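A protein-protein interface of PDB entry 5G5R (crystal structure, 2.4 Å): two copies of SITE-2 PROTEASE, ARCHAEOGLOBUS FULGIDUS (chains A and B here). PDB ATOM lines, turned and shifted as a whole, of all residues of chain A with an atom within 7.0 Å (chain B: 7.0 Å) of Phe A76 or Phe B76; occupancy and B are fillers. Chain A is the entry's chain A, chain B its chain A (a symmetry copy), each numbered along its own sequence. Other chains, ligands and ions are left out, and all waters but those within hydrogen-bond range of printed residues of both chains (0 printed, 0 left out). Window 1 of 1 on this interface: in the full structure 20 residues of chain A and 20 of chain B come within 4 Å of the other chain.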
ATOM      1  N   MET A   1       3.864  18.251 -27.904  1.00  0.00           N
ATOM      2  CA  MET A   1       3.928  18.908 -26.605  1.00  0.00           C
ATOM      3  C   MET A   1       2.904  20.032 -26.501  1.00  0.00           C
ATOM      4  O   MET A   1       2.743  20.825 -27.429  1.00  0.00           O
ATOM      5  CB  MET A   1       5.329  19.461 -26.349  1.00  0.00           C
ATOM      6  CG  MET A   1       5.475  20.156 -25.010  1.00  0.00           C
ATOM      7  SD  MET A   1       7.086  20.923 -24.800  1.00  0.00           S
ATOM      8  CE  MET A   1       8.168  19.502 -24.914  1.00  0.00           C
ATOM      9  N   ASP A   2       2.214  20.096 -25.365  1.00  0.00           N
ATOM     10  CA  ASP A   2       1.244  21.154 -25.146  1.00  0.00           C
ATOM     11  C   ASP A   2       1.950  22.488 -24.913  1.00  0.00           C
ATOM     12  O   ASP A   2       3.148  22.546 -24.619  1.00  0.00           O
ATOM     13  CB  ASP A   2       0.346  20.821 -23.955  1.00  0.00           C
ATOM     14  CG  ASP A   2      -0.406  19.519 -24.141  1.00  0.00           C
ATOM     15  OD1 ASP A   2      -0.536  19.070 -25.299  1.00  0.00           O
ATOM     16  OD2 ASP A   2      -0.871  18.948 -23.131  1.00  0.00           O
ATOM     17  N   VAL A   3       1.177  23.568 -25.047  1.00  0.00           N
ATOM     18  CA  VAL A   3       1.647  24.938 -24.848  1.00  0.00           C
ATOM     19  C   VAL A   3       2.867  25.201 -25.724  1.00  0.00           C
ATOM     20  O   VAL A   3       3.850  25.809 -25.280  1.00  0.00           O
ATOM     21  CB  VAL A   3       1.947  25.216 -23.362  1.00  0.00           C
ATOM     22  CG1 VAL A   3       1.931  26.715 -23.083  1.00  0.00           C
ATOM     23  CG2 VAL A   3       0.936  24.508 -22.475  1.00  0.00           C
ATOM     24  N   GLN A  73       8.145  15.129 -25.724  1.00  0.00           N
ATOM     25  CA  GLN A  73       8.160  15.456 -24.309  1.00  0.00           C
ATOM     26  C   GLN A  73       6.950  16.321 -23.956  1.00  0.00           C
ATOM     27  O   GLN A  73       6.230  16.816 -24.825  1.00  0.00           O
ATOM     28  CB  GLN A  73       9.461  16.164 -23.937  1.00  0.00           C
ATOM     29  CG  GLN A  73      10.711  15.361 -24.259  1.00  0.00           C
ATOM     30  CD  GLN A  73      11.984  16.122 -23.952  1.00  0.00           C
ATOM     31  OE1 GLN A  73      12.734  16.491 -24.856  1.00  0.00           O
ATOM     32  NE2 GLN A  73      12.238  16.358 -22.670  1.00  0.00           N
ATOM     33  N   SER A  74       6.730  16.498 -22.658  1.00  0.00           N
ATOM     34  CA  SER A  74       5.566  17.216 -22.164  1.00  0.00           C
ATOM     35  C   SER A  74       5.926  18.652 -21.814  1.00  0.00           C
ATOM     36  O   SER A  74       7.097  19.007 -21.656  1.00  0.00           O
ATOM     37  CB  SER A  74       4.977  16.518 -20.936  1.00  0.00           C
ATOM     38  OG  SER A  74       5.806  16.711 -19.802  1.00  0.00           O
ATOM     39  N   ALA A  75       4.890  19.484 -21.690  1.00  0.00           N
ATOM     40  CA  ALA A  75       5.099  20.865 -21.278  1.00  0.00           C
ATOM     41  C   ALA A  75       5.651  20.955 -19.863  1.00  0.00           C
ATOM     42  O   ALA A  75       6.284  21.957 -19.514  1.00  0.00           O
ATOM     43  CB  ALA A  75       3.792  21.651 -21.388  1.00  0.00           C
ATOM     44  N   PHE A  76       5.430  19.929 -19.041  1.00  0.00           N
ATOM     45  CA  PHE A  76       5.971  19.929 -17.690  1.00  0.00           C
ATOM     46  C   PHE A  76       7.460  19.614 -17.679  1.00  0.00           C
ATOM     47  O   PHE A  76       8.184  20.100 -16.805  1.00  0.00           O
ATOM     48  CB  PHE A  76       5.192  18.938 -16.826  1.00  0.00           C
ATOM     49  CG  PHE A  76       3.708  19.024 -17.020  1.00  0.00           C
ATOM     50  CD1 PHE A  76       2.999  20.112 -16.543  1.00  0.00           C
ATOM     51  CD2 PHE A  76       3.024  18.032 -17.700  1.00  0.00           C
ATOM     52  CE1 PHE A  76       1.637  20.205 -16.728  1.00  0.00           C
ATOM     53  CE2 PHE A  76       1.659  18.117 -17.888  1.00  0.00           C
ATOM     54  CZ  PHE A  76       0.964  19.206 -17.404  1.00  0.00           C
ATOM     55  N   GLU A  77       7.933  18.813 -18.636  1.00  0.00           N
ATOM     56  CA  GLU A  77       9.371  18.604 -18.770  1.00  0.00           C
ATOM     57  C   GLU A  77      10.061  19.875 -19.246  1.00  0.00           C
ATOM     58  O   GLU A  77      11.142  20.222 -18.753  1.00  0.00           O
ATOM     59  CB  GLU A  77       9.651  17.450 -19.732  1.00  0.00           C
ATOM     60  CG  GLU A  77       8.946  16.155 -19.370  1.00  0.00           C
ATOM     61  CD  GLU A  77       9.158  15.070 -20.407  1.00  0.00           C
ATOM     62  OE1 GLU A  77      10.326  14.778 -20.735  1.00  0.00           O
ATOM     63  OE2 GLU A  77       8.154  14.519 -20.904  1.00  0.00           O
ATOM     64  N   ALA A  78       9.451  20.581 -20.200  1.00  0.00           N
ATOM     65  CA  ALA A  78      10.010  21.850 -20.656  1.00  0.00           C
ATOM     66  C   ALA A  78      10.028  22.875 -19.532  1.00  0.00           C
ATOM     67  O   ALA A  78      10.981  23.653 -19.404  1.00  0.00           O
ATOM     68  CB  ALA A  78       9.216  22.377 -21.852  1.00  0.00           C
ATOM     69  N   PHE A  79       8.980  22.890 -18.703  1.00  0.00           N
ATOM     70  CA  PHE A  79       8.957  23.789 -17.554  1.00  0.00           C
ATOM     71  C   PHE A  79      10.069  23.449 -16.571  1.00  0.00           C
ATOM     72  O   PHE A  79      10.714  24.347 -16.016  1.00  0.00           O
ATOM     73  CB  PHE A  79       7.594  23.722 -16.866  1.00  0.00           C
ATOM     74  CG  PHE A  79       7.434  24.703 -15.742  1.00  0.00           C
ATOM     75  CD1 PHE A  79       7.405  26.065 -15.993  1.00  0.00           C
ATOM     76  CD2 PHE A  79       7.300  24.266 -14.435  1.00  0.00           C
ATOM     77  CE1 PHE A  79       7.255  26.973 -14.961  1.00  0.00           C
ATOM     78  CE2 PHE A  79       7.147  25.170 -13.398  1.00  0.00           C
ATOM     79  CZ  PHE A  79       7.125  26.524 -13.664  1.00  0.00           C
ATOM     80  N   LYS A  80      10.309  22.155 -16.346  1.00  0.00           N
ATOM     81  CA  LYS A  80      11.381  21.745 -15.447  1.00  0.00           C
ATOM     82  C   LYS A  80      12.746  22.144 -15.994  1.00  0.00           C
ATOM     83  O   LYS A  80      13.611  22.607 -15.242  1.00  0.00           O
ATOM     84  CB  LYS A  80      11.313  20.235 -15.213  1.00  0.00           C
ATOM     85  CG  LYS A  80      12.342  19.699 -14.231  1.00  0.00           C
ATOM     86  CD  LYS A  80      13.492  19.017 -14.952  1.00  0.00           C
ATOM     87  CE  LYS A  80      14.420  18.329 -13.968  1.00  0.00           C
ATOM     88  NZ  LYS A  80      15.544  17.642 -14.659  1.00  0.00           N
ATOM     89  N   ILE A  81      12.956  21.974 -17.300  1.00  0.00           N
ATOM     90  CA  ILE A  81      14.244  22.318 -17.891  1.00  0.00           C
ATOM     91  C   ILE A  81      14.473  23.822 -17.836  1.00  0.00           C
ATOM     92  O   ILE A  81      15.566  24.283 -17.486  1.00  0.00           O
ATOM     93  CB  ILE A  81      14.327  21.779 -19.331  1.00  0.00           C
ATOM     94  CG1 ILE A  81      14.321  20.250 -19.319  1.00  0.00           C
ATOM     95  CG2 ILE A  81      15.567  22.309 -20.030  1.00  0.00           C
ATOM     96  CD1 ILE A  81      14.298  19.625 -20.694  1.00  0.00           C
ATOM     97  N   LEU A 107       3.966  29.064 -19.576  1.00  0.00           N
ATOM     98  CA  LEU A 107       3.809  28.049 -18.540  1.00  0.00           C
ATOM     99  C   LEU A 107       3.573  28.671 -17.168  1.00  0.00           C
ATOM    100  O   LEU A 107       2.910  28.061 -16.321  1.00  0.00           O
ATOM    101  CB  LEU A 107       5.034  27.137 -18.514  1.00  0.00           C
ATOM    102  CG  LEU A 107       5.322  26.435 -19.842  1.00  0.00           C
ATOM    103  CD1 LEU A 107       6.550  25.560 -19.731  1.00  0.00           C
ATOM    104  CD2 LEU A 107       4.122  25.617 -20.289  1.00  0.00           C
ATOM    105  N   ILE A 110       0.047  29.267 -17.201  1.00  0.00           N
ATOM    106  CA  ILE A 110      -0.650  27.986 -17.144  1.00  0.00           C
ATOM    107  C   ILE A 110      -0.708  27.470 -15.713  1.00  0.00           C
ATOM    108  O   ILE A 110      -1.681  26.814 -15.317  1.00  0.00           O
ATOM    109  CB  ILE A 110       0.025  26.977 -18.092  1.00  0.00           C
ATOM    110  CG1 ILE A 110      -0.255  27.342 -19.552  1.00  0.00           C
ATOM    111  CG2 ILE A 110      -0.448  25.570 -17.813  1.00  0.00           C
ATOM    112  CD1 ILE A 110      -1.721  27.308 -19.919  1.00  0.00           C
ATOM    113  N   LYS A 111       0.312  27.759 -14.906  1.00  0.00           N
ATOM    114  CA  LYS A 111       0.277  27.314 -13.520  1.00  0.00           C
ATOM    115  C   LYS A 111      -0.781  28.061 -12.718  1.00  0.00           C
ATOM    116  O   LYS A 111      -1.379  27.490 -11.800  1.00  0.00           O
ATOM    117  CB  LYS A 111       1.652  27.483 -12.876  1.00  0.00           C
ATOM    118  CG  LYS A 111       1.798  26.728 -11.571  1.00  0.00           C
ATOM    119  CD  LYS A 111       2.141  27.654 -10.424  1.00  0.00           C
ATOM    120  CE  LYS A 111       2.233  26.880  -9.125  1.00  0.00           C
ATOM    121  NZ  LYS A 111       3.309  25.852  -9.179  1.00  0.00           N
ATOM    122  N   ILE A 113      -3.796  29.342 -13.808  1.00  0.00           N
ATOM    123  CA  ILE A 113      -5.133  28.836 -14.107  1.00  0.00           C
ATOM    124  C   ILE A 113      -5.324  27.446 -13.519  1.00  0.00           C
ATOM    125  O   ILE A 113      -6.440  27.073 -13.135  1.00  0.00           O
ATOM    126  CB  ILE A 113      -5.388  28.863 -15.631  1.00  0.00           C
ATOM    127  CG1 ILE A 113      -6.697  28.153 -15.988  1.00  0.00           C
ATOM    128  CG2 ILE A 113      -4.226  28.254 -16.387  1.00  0.00           C
ATOM    129  CD1 ILE A 113      -7.940  28.835 -15.453  1.00  0.00           C
ATOM    130  N   LEU A 114      -4.246  26.663 -13.414  1.00  0.00           N
ATOM    131  CA  LEU A 114      -4.348  25.363 -12.758  1.00  0.00           C
ATOM    132  C   LEU A 114      -4.745  25.520 -11.296  1.00  0.00           C
ATOM    133  O   LEU A 114      -5.524  24.720 -10.766  1.00  0.00           O
ATOM    134  CB  LEU A 114      -3.025  24.609 -12.880  1.00  0.00           C
ATOM    135  CG  LEU A 114      -3.135  23.199 -13.463  1.00  0.00           C
ATOM    136  CD1 LEU A 114      -3.810  23.245 -14.823  1.00  0.00           C
ATOM    137  CD2 LEU A 114      -1.768  22.543 -13.562  1.00  0.00           C
ATOM    138  N   LEU A 117      -8.311  26.664 -11.582  1.00  0.00           N
ATOM    139  CA  LEU A 117      -9.007  25.402 -11.743  1.00  0.00           C
ATOM    140  C   LEU A 117      -8.889  24.587 -10.457  1.00  0.00           C
ATOM    141  O   LEU A 117      -8.372  25.046  -9.435  1.00  0.00           O
ATOM    142  CB  LEU A 117      -8.432  24.635 -12.931  1.00  0.00           C
ATOM    143  CG  LEU A 117      -9.365  24.280 -14.086  1.00  0.00           C
ATOM    144  CD1 LEU A 117      -8.547  23.880 -15.299  1.00  0.00           C
ATOM    145  CD2 LEU A 117     -10.311  23.160 -13.688  1.00  0.00           C
ATOM    146  N   MET B   1      -1.696  15.256 -27.031  1.00  0.00           N
ATOM    147  CA  MET B   1      -1.955  15.736 -25.679  1.00  0.00           C
ATOM    148  C   MET B   1      -1.014  15.090 -24.670  1.00  0.00           C
ATOM    149  O   MET B   1      -0.780  13.882 -24.711  1.00  0.00           O
ATOM    150  CB  MET B   1      -3.405  15.464 -25.280  1.00  0.00           C
ATOM    151  CG  MET B   1      -3.753  15.943 -23.885  1.00  0.00           C
ATOM    152  SD  MET B   1      -5.416  15.478 -23.388  1.00  0.00           S
ATOM    153  CE  MET B   1      -6.399  16.321 -24.626  1.00  0.00           C
ATOM    154  N   ASP B   2      -0.475  15.902 -23.765  1.00  0.00           N
ATOM    155  CA  ASP B   2       0.402  15.381 -22.731  1.00  0.00           C
ATOM    156  C   ASP B   2      -0.396  14.590 -21.698  1.00  0.00           C
ATOM    157  O   ASP B   2      -1.624  14.698 -21.605  1.00  0.00           O
ATOM    158  CB  ASP B   2       1.163  16.519 -22.049  1.00  0.00           C
ATOM    159  CG  ASP B   2       2.000  17.323 -23.021  1.00  0.00           C
ATOM    160  OD1 ASP B   2       2.297  16.804 -24.117  1.00  0.00           O
ATOM    161  OD2 ASP B   2       2.366  18.471 -22.687  1.00  0.00           O
ATOM    162  N   VAL B   3       0.327  13.789 -20.915  1.00  0.00           N
ATOM    163  CA  VAL B   3      -0.235  12.962 -19.850  1.00  0.00           C
ATOM    164  C   VAL B   3      -1.350  12.083 -20.407  1.00  0.00           C
ATOM    165  O   VAL B   3      -2.411  11.931 -19.789  1.00  0.00           O
ATOM    166  CB  VAL B   3      -0.732  13.825 -18.674  1.00  0.00           C
ATOM    167  CG1 VAL B   3      -0.832  12.993 -17.400  1.00  0.00           C
ATOM    168  CG2 VAL B   3       0.197  15.008 -18.454  1.00  0.00           C
ATOM    169  N   GLN B  73      -6.042  18.757 -28.329  1.00  0.00           N
ATOM    170  CA  GLN B  73      -6.249  19.551 -27.131  1.00  0.00           C
ATOM    171  C   GLN B  73      -5.141  19.273 -26.116  1.00  0.00           C
ATOM    172  O   GLN B  73      -4.346  18.342 -26.261  1.00  0.00           O
ATOM    173  CB  GLN B  73      -7.623  19.260 -26.529  1.00  0.00           C
ATOM    174  CG  GLN B  73      -8.778  19.516 -27.482  1.00  0.00           C
ATOM    175  CD  GLN B  73     -10.119  19.145 -26.883  1.00  0.00           C
ATOM    176  OE1 GLN B  73     -10.769  18.197 -27.326  1.00  0.00           O
ATOM    177  NE2 GLN B  73     -10.542  19.893 -25.871  1.00  0.00           N
ATOM    178  N   SER B  74      -5.094  20.098 -25.077  1.00  0.00           N
ATOM    179  CA  SER B  74      -4.040  20.021 -24.078  1.00  0.00           C
ATOM    180  C   SER B  74      -4.517  19.262 -22.848  1.00  0.00           C
ATOM    181  O   SER B  74      -5.716  19.069 -22.629  1.00  0.00           O
ATOM    182  CB  SER B  74      -3.572  21.420 -23.671  1.00  0.00           C
ATOM    183  OG  SER B  74      -4.544  22.060 -22.862  1.00  0.00           O
ATOM    184  N   ALA B  75      -3.550  18.833 -22.034  1.00  0.00           N
ATOM    185  CA  ALA B  75      -3.882  18.165 -20.784  1.00  0.00           C
ATOM    186  C   ALA B  75      -4.610  19.094 -19.823  1.00  0.00           C
ATOM    187  O   ALA B  75      -5.334  18.620 -18.942  1.00  0.00           O
ATOM    188  CB  ALA B  75      -2.615  17.612 -20.129  1.00  0.00           C
ATOM    189  N   PHE B  76      -4.438  20.407 -19.976  1.00  0.00           N
ATOM    190  CA  PHE B  76      -5.143  21.353 -19.123  1.00  0.00           C
ATOM    191  C   PHE B  76      -6.602  21.499 -19.527  1.00  0.00           C
ATOM    192  O   PHE B  76      -7.454  21.755 -18.672  1.00  0.00           O
ATOM    193  CB  PHE B  76      -4.425  22.702 -19.152  1.00  0.00           C
ATOM    194  CG  PHE B  76      -2.935  22.581 -19.038  1.00  0.00           C
ATOM    195  CD1 PHE B  76      -2.350  22.213 -17.840  1.00  0.00           C
ATOM    196  CD2 PHE B  76      -2.120  22.813 -20.132  1.00  0.00           C
ATOM    197  CE1 PHE B  76      -0.982  22.088 -17.729  1.00  0.00           C
ATOM    198  CE2 PHE B  76      -0.749  22.691 -20.029  1.00  0.00           C
ATOM    199  CZ  PHE B  76      -0.178  22.325 -18.827  1.00  0.00           C
ATOM    200  N   GLU B  77      -6.909  21.337 -20.816  1.00  0.00           N
ATOM    201  CA  GLU B  77      -8.306  21.308 -21.237  1.00  0.00           C
ATOM    202  C   GLU B  77      -8.999  20.050 -20.730  1.00  0.00           C
ATOM    203  O   GLU B  77     -10.149  20.108 -20.278  1.00  0.00           O
ATOM    204  CB  GLU B  77      -8.402  21.396 -22.759  1.00  0.00           C
ATOM    205  CG  GLU B  77      -7.680  22.589 -23.360  1.00  0.00           C
ATOM    206  CD  GLU B  77      -7.703  22.578 -24.875  1.00  0.00           C
ATOM    207  OE1 GLU B  77      -8.805  22.482 -25.454  1.00  0.00           O
ATOM    208  OE2 GLU B  77      -6.617  22.654 -25.486  1.00  0.00           O
ATOM    209  N   ALA B  78      -8.313  18.907 -20.795  1.00  0.00           N
ATOM    210  CA  ALA B  78      -8.877  17.672 -20.260  1.00  0.00           C
ATOM    211  C   ALA B  78      -9.090  17.774 -18.756  1.00  0.00           C
ATOM    212  O   ALA B  78     -10.092  17.279 -18.227  1.00  0.00           O
ATOM    213  CB  ALA B  78      -7.971  16.487 -20.596  1.00  0.00           C
ATOM    214  N   PHE B  79      -8.156  18.418 -18.051  1.00  0.00           N
ATOM    215  CA  PHE B  79      -8.324  18.626 -16.617  1.00  0.00           C
ATOM    216  C   PHE B  79      -9.529  19.511 -16.331  1.00  0.00           C
ATOM    217  O   PHE B  79     -10.286  19.257 -15.385  1.00  0.00           O
ATOM    218  CB  PHE B  79      -7.055  19.241 -16.028  1.00  0.00           C
ATOM    219  CG  PHE B  79      -7.089  19.383 -14.533  1.00  0.00           C
ATOM    220  CD1 PHE B  79      -7.102  18.263 -13.719  1.00  0.00           C
ATOM    221  CD2 PHE B  79      -7.095  20.635 -13.941  1.00  0.00           C
ATOM    222  CE1 PHE B  79      -7.129  18.388 -12.341  1.00  0.00           C
ATOM    223  CE2 PHE B  79      -7.121  20.767 -12.564  1.00  0.00           C
ATOM    224  CZ  PHE B  79      -7.137  19.641 -11.766  1.00  0.00           C
ATOM    225  N   LYS B  80      -9.726  20.553 -17.140  1.00  0.00           N
ATOM    226  CA  LYS B  80     -10.879  21.429 -16.957  1.00  0.00           C
ATOM    227  C   LYS B  80     -12.184  20.686 -17.212  1.00  0.00           C
ATOM    228  O   LYS B  80     -13.160  20.863 -16.473  1.00  0.00           O
ATOM    229  CB  LYS B  80     -10.759  22.644 -17.878  1.00  0.00           C
ATOM    230  CG  LYS B  80     -11.872  23.667 -17.723  1.00  0.00           C
ATOM    231  CD  LYS B  80     -12.886  23.557 -18.849  1.00  0.00           C
ATOM    232  CE  LYS B  80     -13.891  24.692 -18.791  1.00  0.00           C
ATOM    233  NZ  LYS B  80     -14.881  24.608 -19.897  1.00  0.00           N
ATOM    234  N   ILE B  81     -12.220  19.850 -18.251  1.00  0.00           N
ATOM    235  CA  ILE B  81     -13.442  19.117 -18.565  1.00  0.00           C
ATOM    236  C   ILE B  81     -13.756  18.106 -17.471  1.00  0.00           C
ATOM    237  O   ILE B  81     -14.906  17.982 -17.035  1.00  0.00           O
ATOM    238  CB  ILE B  81     -13.317  18.446 -19.945  1.00  0.00           C
ATOM    239  CG1 ILE B  81     -13.230  19.512 -21.039  1.00  0.00           C
ATOM    240  CG2 ILE B  81     -14.486  17.510 -20.193  1.00  0.00           C
ATOM    241  CD1 ILE B  81     -13.002  18.952 -22.424  1.00  0.00           C
ATOM    242  N   LEU B 107      -3.409  13.791 -13.569  1.00  0.00           N
ATOM    243  CA  LEU B 107      -3.327  15.248 -13.576  1.00  0.00           C
ATOM    244  C   LEU B 107      -3.298  15.821 -12.163  1.00  0.00           C
ATOM    245  O   LEU B 107      -2.713  16.888 -11.944  1.00  0.00           O
ATOM    246  CB  LEU B 107      -4.496  15.831 -14.368  1.00  0.00           C
ATOM    247  CG  LEU B 107      -4.578  15.342 -15.815  1.00  0.00           C
ATOM    248  CD1 LEU B 107      -5.763  15.962 -16.523  1.00  0.00           C
ATOM    249  CD2 LEU B 107      -3.290  15.650 -16.560  1.00  0.00           C
ATOM    250  N   ILE B 110       0.168  15.574 -11.317  1.00  0.00           N
ATOM    251  CA  ILE B 110       0.920  16.536 -12.115  1.00  0.00           C
ATOM    252  C   ILE B 110       0.828  17.928 -11.506  1.00  0.00           C
ATOM    253  O   ILE B 110       1.777  18.718 -11.588  1.00  0.00           O
ATOM    254  CB  ILE B 110       0.423  16.513 -13.574  1.00  0.00           C
ATOM    255  CG1 ILE B 110       0.862  15.223 -14.270  1.00  0.00           C
ATOM    256  CG2 ILE B 110       0.932  17.711 -14.340  1.00  0.00           C
ATOM    257  CD1 ILE B 110       2.363  15.060 -14.362  1.00  0.00           C
ATOM    258  N   LYS B 111      -0.299  18.256 -10.875  1.00  0.00           N
ATOM    259  CA  LYS B 111      -0.413  19.566 -10.246  1.00  0.00           C
ATOM    260  C   LYS B 111       0.496  19.683  -9.029  1.00  0.00           C
ATOM    261  O   LYS B 111       1.005  20.772  -8.742  1.00  0.00           O
ATOM    262  CB  LYS B 111      -1.864  19.840  -9.856  1.00  0.00           C
ATOM    263  CG  LYS B 111      -2.131  21.295  -9.530  1.00  0.00           C
ATOM    264  CD  LYS B 111      -2.662  21.464  -8.124  1.00  0.00           C
ATOM    265  CE  LYS B 111      -2.874  22.930  -7.808  1.00  0.00           C
ATOM    266  NZ  LYS B 111      -3.879  23.544  -8.720  1.00  0.00           N
ATOM    267  N   ILE B 113       3.551  18.173  -8.474  1.00  0.00           N
ATOM    268  CA  ILE B 113       4.939  18.379  -8.877  1.00  0.00           C
ATOM    269  C   ILE B 113       5.130  19.774  -9.454  1.00  0.00           C
ATOM    270  O   ILE B 113       6.208  20.367  -9.322  1.00  0.00           O
ATOM    271  CB  ILE B 113       5.380  17.274  -9.863  1.00  0.00           C
ATOM    272  CG1 ILE B 113       6.759  17.577 -10.456  1.00  0.00           C
ATOM    273  CG2 ILE B 113       4.355  17.088 -10.962  1.00  0.00           C
ATOM    274  CD1 ILE B 113       7.888  17.558  -9.445  1.00  0.00           C
ATOM    275  N   LEU B 114       4.091  20.332 -10.081  1.00  0.00           N
ATOM    276  CA  LEU B 114       4.178  21.708 -10.560  1.00  0.00           C
ATOM    277  C   LEU B 114       4.382  22.675  -9.401  1.00  0.00           C
ATOM    278  O   LEU B 114       5.131  23.652  -9.520  1.00  0.00           O
ATOM    279  CB  LEU B 114       2.924  22.070 -11.352  1.00  0.00           C
ATOM    280  CG  LEU B 114       3.180  22.629 -12.752  1.00  0.00           C
ATOM    281  CD1 LEU B 114       4.015  21.652 -13.562  1.00  0.00           C
ATOM    282  CD2 LEU B 114       1.873  22.938 -13.462  1.00  0.00           C
ATOM    283  N   LEU B 117       7.890  21.870  -8.327  1.00  0.00           N
ATOM    284  CA  LEU B 117       8.668  22.661  -9.261  1.00  0.00           C
ATOM    285  C   LEU B 117       8.433  24.146  -8.988  1.00  0.00           C
ATOM    286  O   LEU B 117       7.770  24.538  -8.024  1.00  0.00           O
ATOM    287  CB  LEU B 117       8.285  22.304 -10.695  1.00  0.00           C
ATOM    288  CG  LEU B 117       9.373  21.766 -11.621  1.00  0.00           C
ATOM    289  CD1 LEU B 117       8.735  21.123 -12.839  1.00  0.00           C
ATOM    290  CD2 LEU B 117      10.321  22.877 -12.041  1.00  0.00           C
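Of the 18 printed residues of chain A, 13 touch a printed residue of chain B. Of the 18 printed residues of chain B, 13 touch a printed residue of chain A. Among the printed residues, 23 pairs touch across the chains. Among the printed residues, no Asp or Glu carboxylate lies within 4 Å of a Lys or Arg side-chain nitrogen of the other chain.
The backbone NH (N) of Asp A2 is in hydrogen-bond range of the side-chain carboxylate (OD2) of Asp B2, at 3.1 Å. The side-chain carboxylate (OD2) of Asp A2 sits at hydrogen-bond distance from the backbone NH (N) of Ala B75 (2.9 Å). N of Ala A75 is in hydrogen-bond range of OD2 of Asp B2. NZ of Lys A111 is in hydrogen-bond range of O of Leu B114, 2.9 Å away. NZ of Lys B111 is in hydrogen-bond range of O of Leu A114, at 2.9 Å.
Among the printed residues, pairs that only touch across the chains: Met A1 with Asp B2 (3.6 Å), Asp A2 with Met B1 (3.6 Å), Asp A2 with Gln B73 (3.996 Å), Asp A2 with Ser B74 (3.5 Å), Val A3 with Phe B76 (3.5 Å), Gln A73 with Asp B2 (3.996 Å), Ser A74 with Asp B2 (3.5 Å), Phe A76 with Val B3 (3.5 Å), Phe A76 with Phe B76 (3.4 Å), Phe A76 with Ile B110 (3.4 Å), Phe A76 with Leu B114 (3.5 Å), Phe A79 with Leu B117 (3.8 Å), Lys A80 with Leu B117 (3.6 Å), Ile A110 with Phe B76 (3.4 Å), Leu A114 with Phe B76 (3.5 Å), Leu A114 with Leu B114 (3.7 Å), Leu A117 with Phe B79 (3.8 Å) and Leu A117 with Lys B80 (3.6 Å).
OE1 of Glu A77 is in hydrogen-bond range of NE2 of Gln A73, at 3.1 Å. OG of Ser A74 lies close to N of Phe A76, at 3.3 Å. The backbone NH of Ser A74 is in hydrogen-bond range of the side-chain carboxylate of Glu A77 (3.0 Å). OE1 of Glu B77 sits at hydrogen-bond distance from NE2 of Gln B73, 3.1 Å away. N of Phe B76 sits close to OG of Ser B74 (3.3 Å). The backbone NH (N) of Ser B74 lies within hydrogen-bond range of the side-chain carboxylate (OE2) of Glu B77 (3.0 Å).
Of chain B, only Val B3, Phe B76, Ile B110 and Leu B114 come within 4 Å of Phe A76. Phe B76 touches just these residues of chain A: Val A3 (3.5 Å), Phe A76 (3.4 Å), Ile A110 (3.4 Å) and Leu A114 (3.5 Å). Of the printed residues of chain B, Met A1 touches Asp B2. Printed residues of chain A within 4 Å of Ile B110: Phe A76. Of the printed residues of chain A, Leu B117 touches Phe A79 (3.8 Å) and Lys A80 (3.6 Å). Printed residues of chain B within 4 Å of Asp A2: Met B1, Asp B2, Gln B73, Ser B74 and Ala B75. Glu B77 touches none of the printed residues of chain A. Ile B113 touches none of the printed residues of chain A. The nearest residue of chain B that does not touch Phe A76 is Leu B117 (4.1 Å). The nearest residue of chain A that does not touch Phe B76 is Leu A117 (4.1 Å). The nearest printed residue of chain B that does not touch Lys A80 is Ile B113 (6.9 Å).
Met A1 touches Asp B2, and with the chains exchanged Asp A2 touches Met B1. Phe B76 touches its own counterpart, Phe A76. Phe A76 touches Ile B110, and with the chains exchanged Ile A110 touches Phe B76. Phe A76 touches Leu B114, and with the chains exchanged Leu A114 touches Phe B76.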
